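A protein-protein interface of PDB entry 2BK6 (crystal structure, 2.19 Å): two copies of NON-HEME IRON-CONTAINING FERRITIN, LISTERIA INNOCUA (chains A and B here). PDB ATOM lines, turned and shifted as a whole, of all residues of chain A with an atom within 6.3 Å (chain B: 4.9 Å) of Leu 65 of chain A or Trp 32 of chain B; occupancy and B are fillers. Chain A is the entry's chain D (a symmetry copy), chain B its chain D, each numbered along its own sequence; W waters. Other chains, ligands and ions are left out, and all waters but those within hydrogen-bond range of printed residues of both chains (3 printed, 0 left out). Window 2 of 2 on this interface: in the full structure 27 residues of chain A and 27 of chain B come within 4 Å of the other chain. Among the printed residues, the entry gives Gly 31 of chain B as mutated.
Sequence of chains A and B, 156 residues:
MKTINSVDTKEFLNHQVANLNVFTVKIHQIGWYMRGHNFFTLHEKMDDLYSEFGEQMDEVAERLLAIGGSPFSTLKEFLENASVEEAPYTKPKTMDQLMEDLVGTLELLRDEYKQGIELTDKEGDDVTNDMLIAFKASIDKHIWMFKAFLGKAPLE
The side-chain hydroxyl of Tyr 33 of chain B sits close to the backbone carbonyl oxygen of Pro 71 of chain A (2.4 Å).
OE2 of Glu 62 of chain A lies close to NE2 of His 43 of chain B.
NE1 of Trp 32 of chain B lies within hydrogen-bond range of OD1 of Asp 58 of chain A.
The side-chain amide oxygen (OE1) of Gln 29 of chain B is in hydrogen-bond range of the side-chain hydroxyl (OG) of Ser 73 of chain A (3.1 Å).
N of His 43 of chain B lies within hydrogen-bond range of SD of Met 34 of chain B (3.3 Å).
SD of Met 57 of chain A lies close to ND2 of Asn 21 of chain A (3.3 Å).
The backbone carbonyl oxygen (O) of Gly 31 of chain B sits at hydrogen-bond distance from a ring nitrogen (ND1) of His 43 of chain B, 2.8 Å away.
Among the printed residues, merely in contact across the chains: Met 57 of chain A with His 28 of chain B, Met 57 of chain A with Trp 32 of chain B, Asp 58 of chain A with His 28 of chain B, Ala 61 of chain A with Trp 32 of chain B, Glu 62 of chain A with Trp 32 of chain B, Leu 65 of chain A with Trp 32 of chain B, Ser 70 of chain A with Tyr 33 of chain B, Pro 71 of chain A with Trp 32 of chain B, Phe 72 of chain A with Trp 32 of chain B, Ser 73 of chain A with Trp 32 of chain B and Ser 73 of chain A with Tyr 33 of chain B.
Of chain B, only Trp 32 (3.6 Å) comes within 4 Å of Leu 65 of chain A.
Printed residues of chain B within 4 Å of Ser 73 of chain A: Gln 29 (3.1 Å), Trp 32 (3.98 Å) and Tyr 33 (3.4 Å).
Of the printed residues of chain B, Ser 70 of chain A touches Tyr 33.
Met 34 of chain B touches none of the printed residues of chain A.
Gly 31 of chain B touches none of the printed residues of chain A.
The nearest residue of chain B that does not touch Leu 65 of chain A is Tyr 33 of chain B (4.6 Å).
The nearest printed residue of chain B that does not touch Ala 61 of chain A is His 28 of chain B (6.7 Å).
Of the 19 printed residues of chain A, 9 touch a printed residue of chain B.
No position is printed for both chains.
Of the 15 pairs that touch across the chains among the printed residues, none has its exchanged pair printed and touching as well.
Water W3 lies within hydrogen-bond range of the side-chain carboxylate of Glu 62 of chain A (2.6 Å), the side-chain carboxylate of Asp 58 of chain A (2.7 Å) and the indole nitrogen of Trp 32 of chain B (3.4 Å).
Water W2 lies within hydrogen-bond range of a ring nitrogen (NE2) of His 43 of chain B (2.6 Å) and the side-chain carboxylate (OE1) of Glu 62 of chain A (2.8 Å).
Water W1 lies within hydrogen-bond range of the backbone carbonyl oxygen (O) of Ser 73 of chain A (2.8 Å) and the side-chain amide oxygen (OE1) of Gln 29 of chain B (3.2 Å).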
ATOM      1  N   VAL A  17      30.917   0.142  27.352  1.00  0.00           N
ATOM      2  CA  VAL A  17      30.120  -0.346  26.186  1.00  0.00           C
ATOM      3  C   VAL A  17      29.388   0.879  25.580  1.00  0.00           C
ATOM      4  O   VAL A  17      29.437   1.099  24.356  1.00  0.00           O
ATOM      5  CB  VAL A  17      29.102  -1.479  26.532  1.00  0.00           C
ATOM      6  CG1 VAL A  17      28.264  -1.892  25.295  1.00  0.00           C
ATOM      7  CG2 VAL A  17      29.813  -2.708  27.072  1.00  0.00           C
ATOM      8  N   ASN A  21      30.584   2.898  21.947  1.00  0.00           N
ATOM      9  CA  ASN A  21      29.566   3.024  20.916  1.00  0.00           C
ATOM     10  C   ASN A  21      29.335   4.465  20.499  1.00  0.00           C
ATOM     11  O   ASN A  21      29.082   4.714  19.326  1.00  0.00           O
ATOM     12  CB  ASN A  21      28.283   2.334  21.319  1.00  0.00           C
ATOM     13  CG  ASN A  21      28.291   0.858  20.974  1.00  0.00           C
ATOM     14  OD1 ASN A  21      28.041   0.472  19.826  1.00  0.00           O
ATOM     15  ND2 ASN A  21      28.516   0.019  21.975  1.00  0.00           N
ATOM     16  N   MET A  57      35.129  -2.456  22.165  1.00  0.00           N
ATOM     17  CA  MET A  57      33.732  -2.418  22.601  1.00  0.00           C
ATOM     18  C   MET A  57      33.167  -3.816  22.753  1.00  0.00           C
ATOM     19  O   MET A  57      32.625  -4.141  23.806  1.00  0.00           O
ATOM     20  CB  MET A  57      32.905  -1.547  21.637  1.00  0.00           C
ATOM     21  CG  MET A  57      31.466  -1.297  22.044  1.00  0.00           C
ATOM     22  SD  MET A  57      30.367  -2.674  21.744  1.00  0.00           S
ATOM     23  CE  MET A  57      30.190  -2.623  19.962  1.00  0.00           C
ATOM     24  N   ASP A  58      33.315  -4.626  21.704  1.00  0.00           N
ATOM     25  CA  ASP A  58      32.833  -5.996  21.690  1.00  0.00           C
ATOM     26  C   ASP A  58      33.515  -6.838  22.775  1.00  0.00           C
ATOM     27  O   ASP A  58      32.848  -7.607  23.454  1.00  0.00           O
ATOM     28  CB  ASP A  58      32.999  -6.613  20.301  1.00  0.00           C
ATOM     29  CG  ASP A  58      32.165  -7.866  20.120  1.00  0.00           C
ATOM     30  OD1 ASP A  58      31.015  -7.936  20.619  1.00  0.00           O
ATOM     31  OD2 ASP A  58      32.640  -8.799  19.451  1.00  0.00           O
ATOM     32  N   VAL A  60      34.887  -5.643  25.594  1.00  0.00           N
ATOM     33  CA  VAL A  60      34.354  -5.100  26.871  1.00  0.00           C
ATOM     34  C   VAL A  60      33.006  -5.773  27.182  1.00  0.00           C
ATOM     35  O   VAL A  60      32.827  -6.329  28.284  1.00  0.00           O
ATOM     36  CB  VAL A  60      34.264  -3.517  26.878  1.00  0.00           C
ATOM     37  CG1 VAL A  60      33.448  -2.974  28.039  1.00  0.00           C
ATOM     38  CG2 VAL A  60      35.644  -2.860  26.935  1.00  0.00           C
ATOM     39  N   ALA A  61      32.102  -5.751  26.198  1.00  0.00           N
ATOM     40  CA  ALA A  61      30.765  -6.338  26.305  1.00  0.00           C
ATOM     41  C   ALA A  61      30.779  -7.849  26.560  1.00  0.00           C
ATOM     42  O   ALA A  61      29.989  -8.359  27.361  1.00  0.00           O
ATOM     43  CB  ALA A  61      30.002  -6.022  25.097  1.00  0.00           C
ATOM     44  N   GLU A  62      31.681  -8.550  25.887  1.00  0.00           N
ATOM     45  CA  GLU A  62      31.838 -10.004  26.056  1.00  0.00           C
ATOM     46  C   GLU A  62      32.549 -10.366  27.358  1.00  0.00           C
ATOM     47  O   GLU A  62      32.282 -11.438  27.917  1.00  0.00           O
ATOM     48  CB  GLU A  62      32.479 -10.646  24.833  1.00  0.00           C
ATOM     49  CG  GLU A  62      31.498 -10.626  23.652  1.00  0.00           C
ATOM     50  CD  GLU A  62      31.936 -11.394  22.414  1.00  0.00           C
ATOM     51  OE1 GLU A  62      33.078 -11.922  22.339  1.00  0.00           O
ATOM     52  OE2 GLU A  62      31.097 -11.439  21.493  1.00  0.00           O
ATOM     53  N   ARG A  63      33.441  -9.487  27.825  1.00  0.00           N
ATOM     54  CA  ARG A  63      34.069  -9.646  29.149  1.00  0.00           C
ATOM     55  C   ARG A  63      32.981  -9.490  30.225  1.00  0.00           C
ATOM     56  O   ARG A  63      32.929 -10.296  31.153  1.00  0.00           O
ATOM     57  CB  ARG A  63      35.228  -8.671  29.389  1.00  0.00           C
ATOM     58  CG  ARG A  63      35.931  -8.757  30.773  1.00  0.00           C
ATOM     59  CD  ARG A  63      36.485 -10.167  31.083  1.00  0.00           C
ATOM     60  NE  ARG A  63      36.778 -10.351  32.510  1.00  0.00           N
ATOM     61  CZ  ARG A  63      36.918 -11.531  33.111  1.00  0.00           C
ATOM     62  NH1 ARG A  63      36.784 -12.671  32.430  1.00  0.00           N
ATOM     63  NH2 ARG A  63      37.194 -11.573  34.409  1.00  0.00           N
ATOM     64  N   LEU A  64      32.124  -8.477  30.057  1.00  0.00           N
ATOM     65  CA  LEU A  64      30.992  -8.214  30.934  1.00  0.00           C
ATOM     66  C   LEU A  64      30.095  -9.437  31.036  1.00  0.00           C
ATOM     67  O   LEU A  64      29.747  -9.846  32.151  1.00  0.00           O
ATOM     68  CB  LEU A  64      30.217  -6.977  30.471  1.00  0.00           C
ATOM     69  CG  LEU A  64      28.959  -6.542  31.238  1.00  0.00           C
ATOM     70  CD1 LEU A  64      29.236  -6.333  32.720  1.00  0.00           C
ATOM     71  CD2 LEU A  64      28.500  -5.255  30.638  1.00  0.00           C
ATOM     72  N   LEU A  65      29.748 -10.011  29.874  1.00  0.00           N
ATOM     73  CA  LEU A  65      29.007 -11.273  29.767  1.00  0.00           C
ATOM     74  C   LEU A  65      29.642 -12.402  30.559  1.00  0.00           C
ATOM     75  O   LEU A  65      28.936 -13.076  31.301  1.00  0.00           O
ATOM     76  CB  LEU A  65      28.908 -11.670  28.302  1.00  0.00           C
ATOM     77  CG  LEU A  65      27.671 -11.586  27.397  1.00  0.00           C
ATOM     78  CD1 LEU A  65      26.334 -11.033  27.946  1.00  0.00           C
ATOM     79  CD2 LEU A  65      28.116 -10.971  26.099  1.00  0.00           C
ATOM     80  N   ALA A  66      30.965 -12.577  30.393  1.00  0.00           N
ATOM     81  CA  ALA A  66      31.786 -13.599  31.080  1.00  0.00           C
ATOM     82  C   ALA A  66      31.820 -13.453  32.600  1.00  0.00           C
ATOM     83  O   ALA A  66      32.018 -14.451  33.309  1.00  0.00           O
ATOM     84  CB  ALA A  66      33.206 -13.601  30.537  1.00  0.00           C
ATOM     85  N   ILE A  67      31.643 -12.221  33.093  1.00  0.00           N
ATOM     86  CA  ILE A  67      31.592 -11.955  34.545  1.00  0.00           C
ATOM     87  C   ILE A  67      30.155 -11.911  35.133  1.00  0.00           C
ATOM     88  O   ILE A  67      29.965 -11.477  36.269  1.00  0.00           O
ATOM     89  CB  ILE A  67      32.480 -10.740  34.990  1.00  0.00           C
ATOM     90  CG1 ILE A  67      31.947  -9.410  34.438  1.00  0.00           C
ATOM     91  CG2 ILE A  67      33.924 -11.007  34.628  1.00  0.00           C
ATOM     92  CD1 ILE A  67      32.643  -8.160  34.965  1.00  0.00           C
ATOM     93  N   GLY A  68      29.176 -12.381  34.358  1.00  0.00           N
ATOM     94  CA  GLY A  68      27.769 -12.453  34.772  1.00  0.00           C
ATOM     95  C   GLY A  68      26.972 -11.167  34.591  1.00  0.00           C
ATOM     96  O   GLY A  68      25.874 -11.024  35.149  1.00  0.00           O
ATOM     97  N   GLY A  69      27.528 -10.228  33.823  1.00  0.00           N
ATOM     98  CA  GLY A  69      26.867  -8.973  33.527  1.00  0.00           C
ATOM     99  C   GLY A  69      25.923  -9.036  32.348  1.00  0.00           C
ATOM    100  O   GLY A  69      25.837 -10.057  31.639  1.00  0.00           O
ATOM    101  N   SER A  70      25.215  -7.921  32.171  1.00  0.00           N
ATOM    102  CA  SER A  70      24.235  -7.712  31.113  1.00  0.00           C
ATOM    103  C   SER A  70      24.603  -6.419  30.381  1.00  0.00           C
ATOM    104  O   SER A  70      24.323  -5.329  30.892  1.00  0.00           O
ATOM    105  CB  SER A  70      22.816  -7.638  31.692  1.00  0.00           C
ATOM    106  OG  SER A  70      22.431  -8.898  32.193  1.00  0.00           O
ATOM    107  N   PRO A  71      25.289  -6.527  29.212  1.00  0.00           N
ATOM    108  CA  PRO A  71      25.663  -5.299  28.480  1.00  0.00           C
ATOM    109  C   PRO A  71      24.495  -4.508  27.895  1.00  0.00           C
ATOM    110  O   PRO A  71      23.497  -5.101  27.464  1.00  0.00           O
ATOM    111  CB  PRO A  71      26.585  -5.809  27.356  1.00  0.00           C
ATOM    112  CG  PRO A  71      26.237  -7.249  27.183  1.00  0.00           C
ATOM    113  CD  PRO A  71      25.796  -7.735  28.531  1.00  0.00           C
ATOM    114  N   PHE A  72      24.634  -3.181  27.913  1.00  0.00           N
ATOM    115  CA  PHE A  72      23.724  -2.287  27.220  1.00  0.00           C
ATOM    116  C   PHE A  72      23.812  -2.688  25.754  1.00  0.00           C
ATOM    117  O   PHE A  72      24.905  -2.991  25.244  1.00  0.00           O
ATOM    118  CB  PHE A  72      24.127  -0.823  27.394  1.00  0.00           C
ATOM    119  CG  PHE A  72      24.114  -0.339  28.830  1.00  0.00           C
ATOM    120  CD1 PHE A  72      23.007  -0.592  29.683  1.00  0.00           C
ATOM    121  CD2 PHE A  72      25.178   0.441  29.310  1.00  0.00           C
ATOM    122  CE1 PHE A  72      22.999  -0.118  31.021  1.00  0.00           C
ATOM    123  CE2 PHE A  72      25.191   0.930  30.647  1.00  0.00           C
ATOM    124  CZ  PHE A  72      24.100   0.655  31.505  1.00  0.00           C
ATOM    125  N   SER A  73      22.665  -2.762  25.094  1.00  0.00           N
ATOM    126  CA  SER A  73      22.644  -3.247  23.713  1.00  0.00           C
ATOM    127  C   SER A  73      21.607  -2.563  22.838  1.00  0.00           C
ATOM    128  O   SER A  73      21.029  -3.170  21.941  1.00  0.00           O
ATOM    129  CB  SER A  73      22.546  -4.772  23.697  1.00  0.00           C
ATOM    130  OG  SER A  73      21.342  -5.182  24.295  1.00  0.00           O
ATOM    131  N   PHE A  78      22.974   3.320  25.342  1.00  0.00           N
ATOM    132  CA  PHE A  78      24.311   3.924  25.192  1.00  0.00           C
ATOM    133  C   PHE A  78      24.261   5.429  25.442  1.00  0.00           C
ATOM    134  O   PHE A  78      25.117   5.946  26.156  1.00  0.00           O
ATOM    135  CB  PHE A  78      25.012   3.648  23.845  1.00  0.00           C
ATOM    136  CG  PHE A  78      25.024   2.206  23.403  1.00  0.00           C
ATOM    137  CD1 PHE A  78      25.302   1.147  24.294  1.00  0.00           C
ATOM    138  CD2 PHE A  78      24.837   1.916  22.042  1.00  0.00           C
ATOM    139  CE1 PHE A  78      25.321  -0.188  23.840  1.00  0.00           C
ATOM    140  CE2 PHE A  78      24.865   0.596  21.576  1.00  0.00           C
ATOM    141  CZ  PHE A  78      25.114  -0.468  22.474  1.00  0.00           C
ATOM    142  N   HIS B  28      24.458  -7.266  17.602  1.00  0.00           N
ATOM    143  CA  HIS B  28      25.289  -7.477  18.796  1.00  0.00           C
ATOM    144  C   HIS B  28      24.478  -7.935  19.989  1.00  0.00           C
ATOM    145  O   HIS B  28      24.893  -8.870  20.650  1.00  0.00           O
ATOM    146  CB  HIS B  28      26.168  -6.284  19.145  1.00  0.00           C
ATOM    147  CG  HIS B  28      27.530  -6.319  18.523  1.00  0.00           C
ATOM    148  ND1 HIS B  28      28.031  -7.418  17.845  1.00  0.00           N
ATOM    149  CD2 HIS B  28      28.559  -5.448  18.627  1.00  0.00           C
ATOM    150  CE1 HIS B  28      29.272  -7.174  17.472  1.00  0.00           C
ATOM    151  NE2 HIS B  28      29.617  -5.984  17.934  1.00  0.00           N
ATOM    152  N   GLN B  29      23.312  -7.314  20.226  1.00  0.00           N
ATOM    153  CA  GLN B  29      22.374  -7.738  21.301  1.00  0.00           C
ATOM    154  C   GLN B  29      22.072  -9.239  21.177  1.00  0.00           C
ATOM    155  O   GLN B  29      22.243  -9.989  22.143  1.00  0.00           O
ATOM    156  CB  GLN B  29      21.060  -6.929  21.243  1.00  0.00           C
ATOM    157  CG  GLN B  29      19.986  -7.364  22.247  1.00  0.00           C
ATOM    158  CD  GLN B  29      18.752  -6.521  22.152  1.00  0.00           C
ATOM    159  OE1 GLN B  29      18.723  -5.398  22.652  1.00  0.00           O
ATOM    160  NE2 GLN B  29      17.711  -7.062  21.529  1.00  0.00           N
ATOM    161  N   ILE B  30      21.660  -9.642  19.975  1.00  0.00           N
ATOM    162  CA  ILE B  30      21.333 -11.017  19.647  1.00  0.00           C
ATOM    163  C   ILE B  30      22.563 -11.928  19.884  1.00  0.00           C
ATOM    164  O   ILE B  30      22.444 -12.908  20.603  1.00  0.00           O
ATOM    165  CB  ILE B  30      20.730 -11.122  18.224  1.00  0.00           C
ATOM    166  CG1 ILE B  30      19.400 -10.321  18.134  1.00  0.00           C
ATOM    167  CG2 ILE B  30      20.535 -12.579  17.874  1.00  0.00           C
ATOM    168  CD1 ILE B  30      18.746 -10.172  16.699  1.00  0.00           C
ATOM    169  N   GLY B  31      23.724 -11.561  19.325  1.00  0.00           N
ATOM    170  CA  GLY B  31      24.966 -12.331  19.512  1.00  0.00           C
ATOM    171  C   GLY B  31      25.438 -12.449  20.959  1.00  0.00           C
ATOM    172  O   GLY B  31      25.982 -13.480  21.344  1.00  0.00           O
ATOM    173  N   TRP B  32      25.222 -11.391  21.746  1.00  0.00           N
ATOM    174  CA  TRP B  32      25.602 -11.353  23.163  1.00  0.00           C
ATOM    175  C   TRP B  32      24.704 -12.146  24.075  1.00  0.00           C
ATOM    176  O   TRP B  32      25.202 -12.925  24.899  1.00  0.00           O
ATOM    177  CB  TRP B  32      25.721  -9.916  23.688  1.00  0.00           C
ATOM    178  CG  TRP B  32      26.792  -9.097  23.026  1.00  0.00           C
ATOM    179  CD1 TRP B  32      27.916  -9.563  22.396  1.00  0.00           C
ATOM    180  CD2 TRP B  32      26.885  -7.663  23.008  1.00  0.00           C
ATOM    181  NE1 TRP B  32      28.670  -8.515  21.933  1.00  0.00           N
ATOM    182  CE2 TRP B  32      28.079  -7.335  22.301  1.00  0.00           C
ATOM    183  CE3 TRP B  32      26.069  -6.619  23.495  1.00  0.00           C
ATOM    184  CZ2 TRP B  32      28.471  -6.015  22.062  1.00  0.00           C
ATOM    185  CZ3 TRP B  32      26.470  -5.290  23.270  1.00  0.00           C
ATOM    186  CH2 TRP B  32      27.662  -5.005  22.555  1.00  0.00           C
ATOM    187  N   TYR B  33      23.394 -11.968  23.910  1.00  0.00           N
ATOM    188  CA  TYR B  33      22.392 -12.583  24.788  1.00  0.00           C
ATOM    189  C   TYR B  33      21.874 -13.973  24.436  1.00  0.00           C
ATOM    190  O   TYR B  33      21.269 -14.636  25.298  1.00  0.00           O
ATOM    191  CB  TYR B  33      21.231 -11.622  25.002  1.00  0.00           C
ATOM    192  CG  TYR B  33      21.582 -10.427  25.852  1.00  0.00           C
ATOM    193  CD1 TYR B  33      21.691 -10.546  27.259  1.00  0.00           C
ATOM    194  CD2 TYR B  33      21.796  -9.163  25.261  1.00  0.00           C
ATOM    195  CE1 TYR B  33      22.019  -9.423  28.063  1.00  0.00           C
ATOM    196  CE2 TYR B  33      22.115  -8.035  26.053  1.00  0.00           C
ATOM    197  CZ  TYR B  33      22.223  -8.186  27.450  1.00  0.00           C
ATOM    198  OH  TYR B  33      22.523  -7.102  28.225  1.00  0.00           O
ATOM    199  N   MET B  34      22.112 -14.413  23.199  1.00  0.00           N
ATOM    200  CA  MET B  34      21.684 -15.747  22.737  1.00  0.00           C
ATOM    201  C   MET B  34      22.219 -16.891  23.579  1.00  0.00           C
ATOM    202  O   MET B  34      23.362 -16.845  24.062  1.00  0.00           O
ATOM    203  CB  MET B  34      22.052 -15.983  21.264  1.00  0.00           C
ATOM    204  CG  MET B  34      23.549 -15.837  20.908  1.00  0.00           C
ATOM    205  SD  MET B  34      23.995 -16.690  19.401  1.00  0.00           S
ATOM    206  CE  MET B  34      23.015 -15.769  18.211  1.00  0.00           C
ATOM    207  N   HIS B  43      26.222 -17.300  17.022  1.00  0.00           N
ATOM    208  CA  HIS B  43      27.029 -16.207  17.579  1.00  0.00           C
ATOM    209  C   HIS B  43      28.037 -15.717  16.518  1.00  0.00           C
ATOM    210  O   HIS B  43      28.160 -14.524  16.305  1.00  0.00           O
ATOM    211  CB  HIS B  43      27.730 -16.607  18.874  1.00  0.00           C
ATOM    212  CG  HIS B  43      28.665 -15.562  19.378  1.00  0.00           C
ATOM    213  ND1 HIS B  43      28.229 -14.441  20.048  1.00  0.00           N
ATOM    214  CD2 HIS B  43      30.008 -15.447  19.277  1.00  0.00           C
ATOM    215  CE1 HIS B  43      29.266 -13.686  20.357  1.00  0.00           C
ATOM    216  NE2 HIS B  43      30.356 -14.269  19.888  1.00  0.00           N
HETATM  217  O   HOH W   1      19.001  -3.566  20.066  1.00  0.00           O
HETATM  218  O   HOH W   2      32.798 -13.263  19.898  1.00  0.00           O
HETATM  219  O   HOH W   3      30.181 -10.181  19.426  1.00  0.00           O
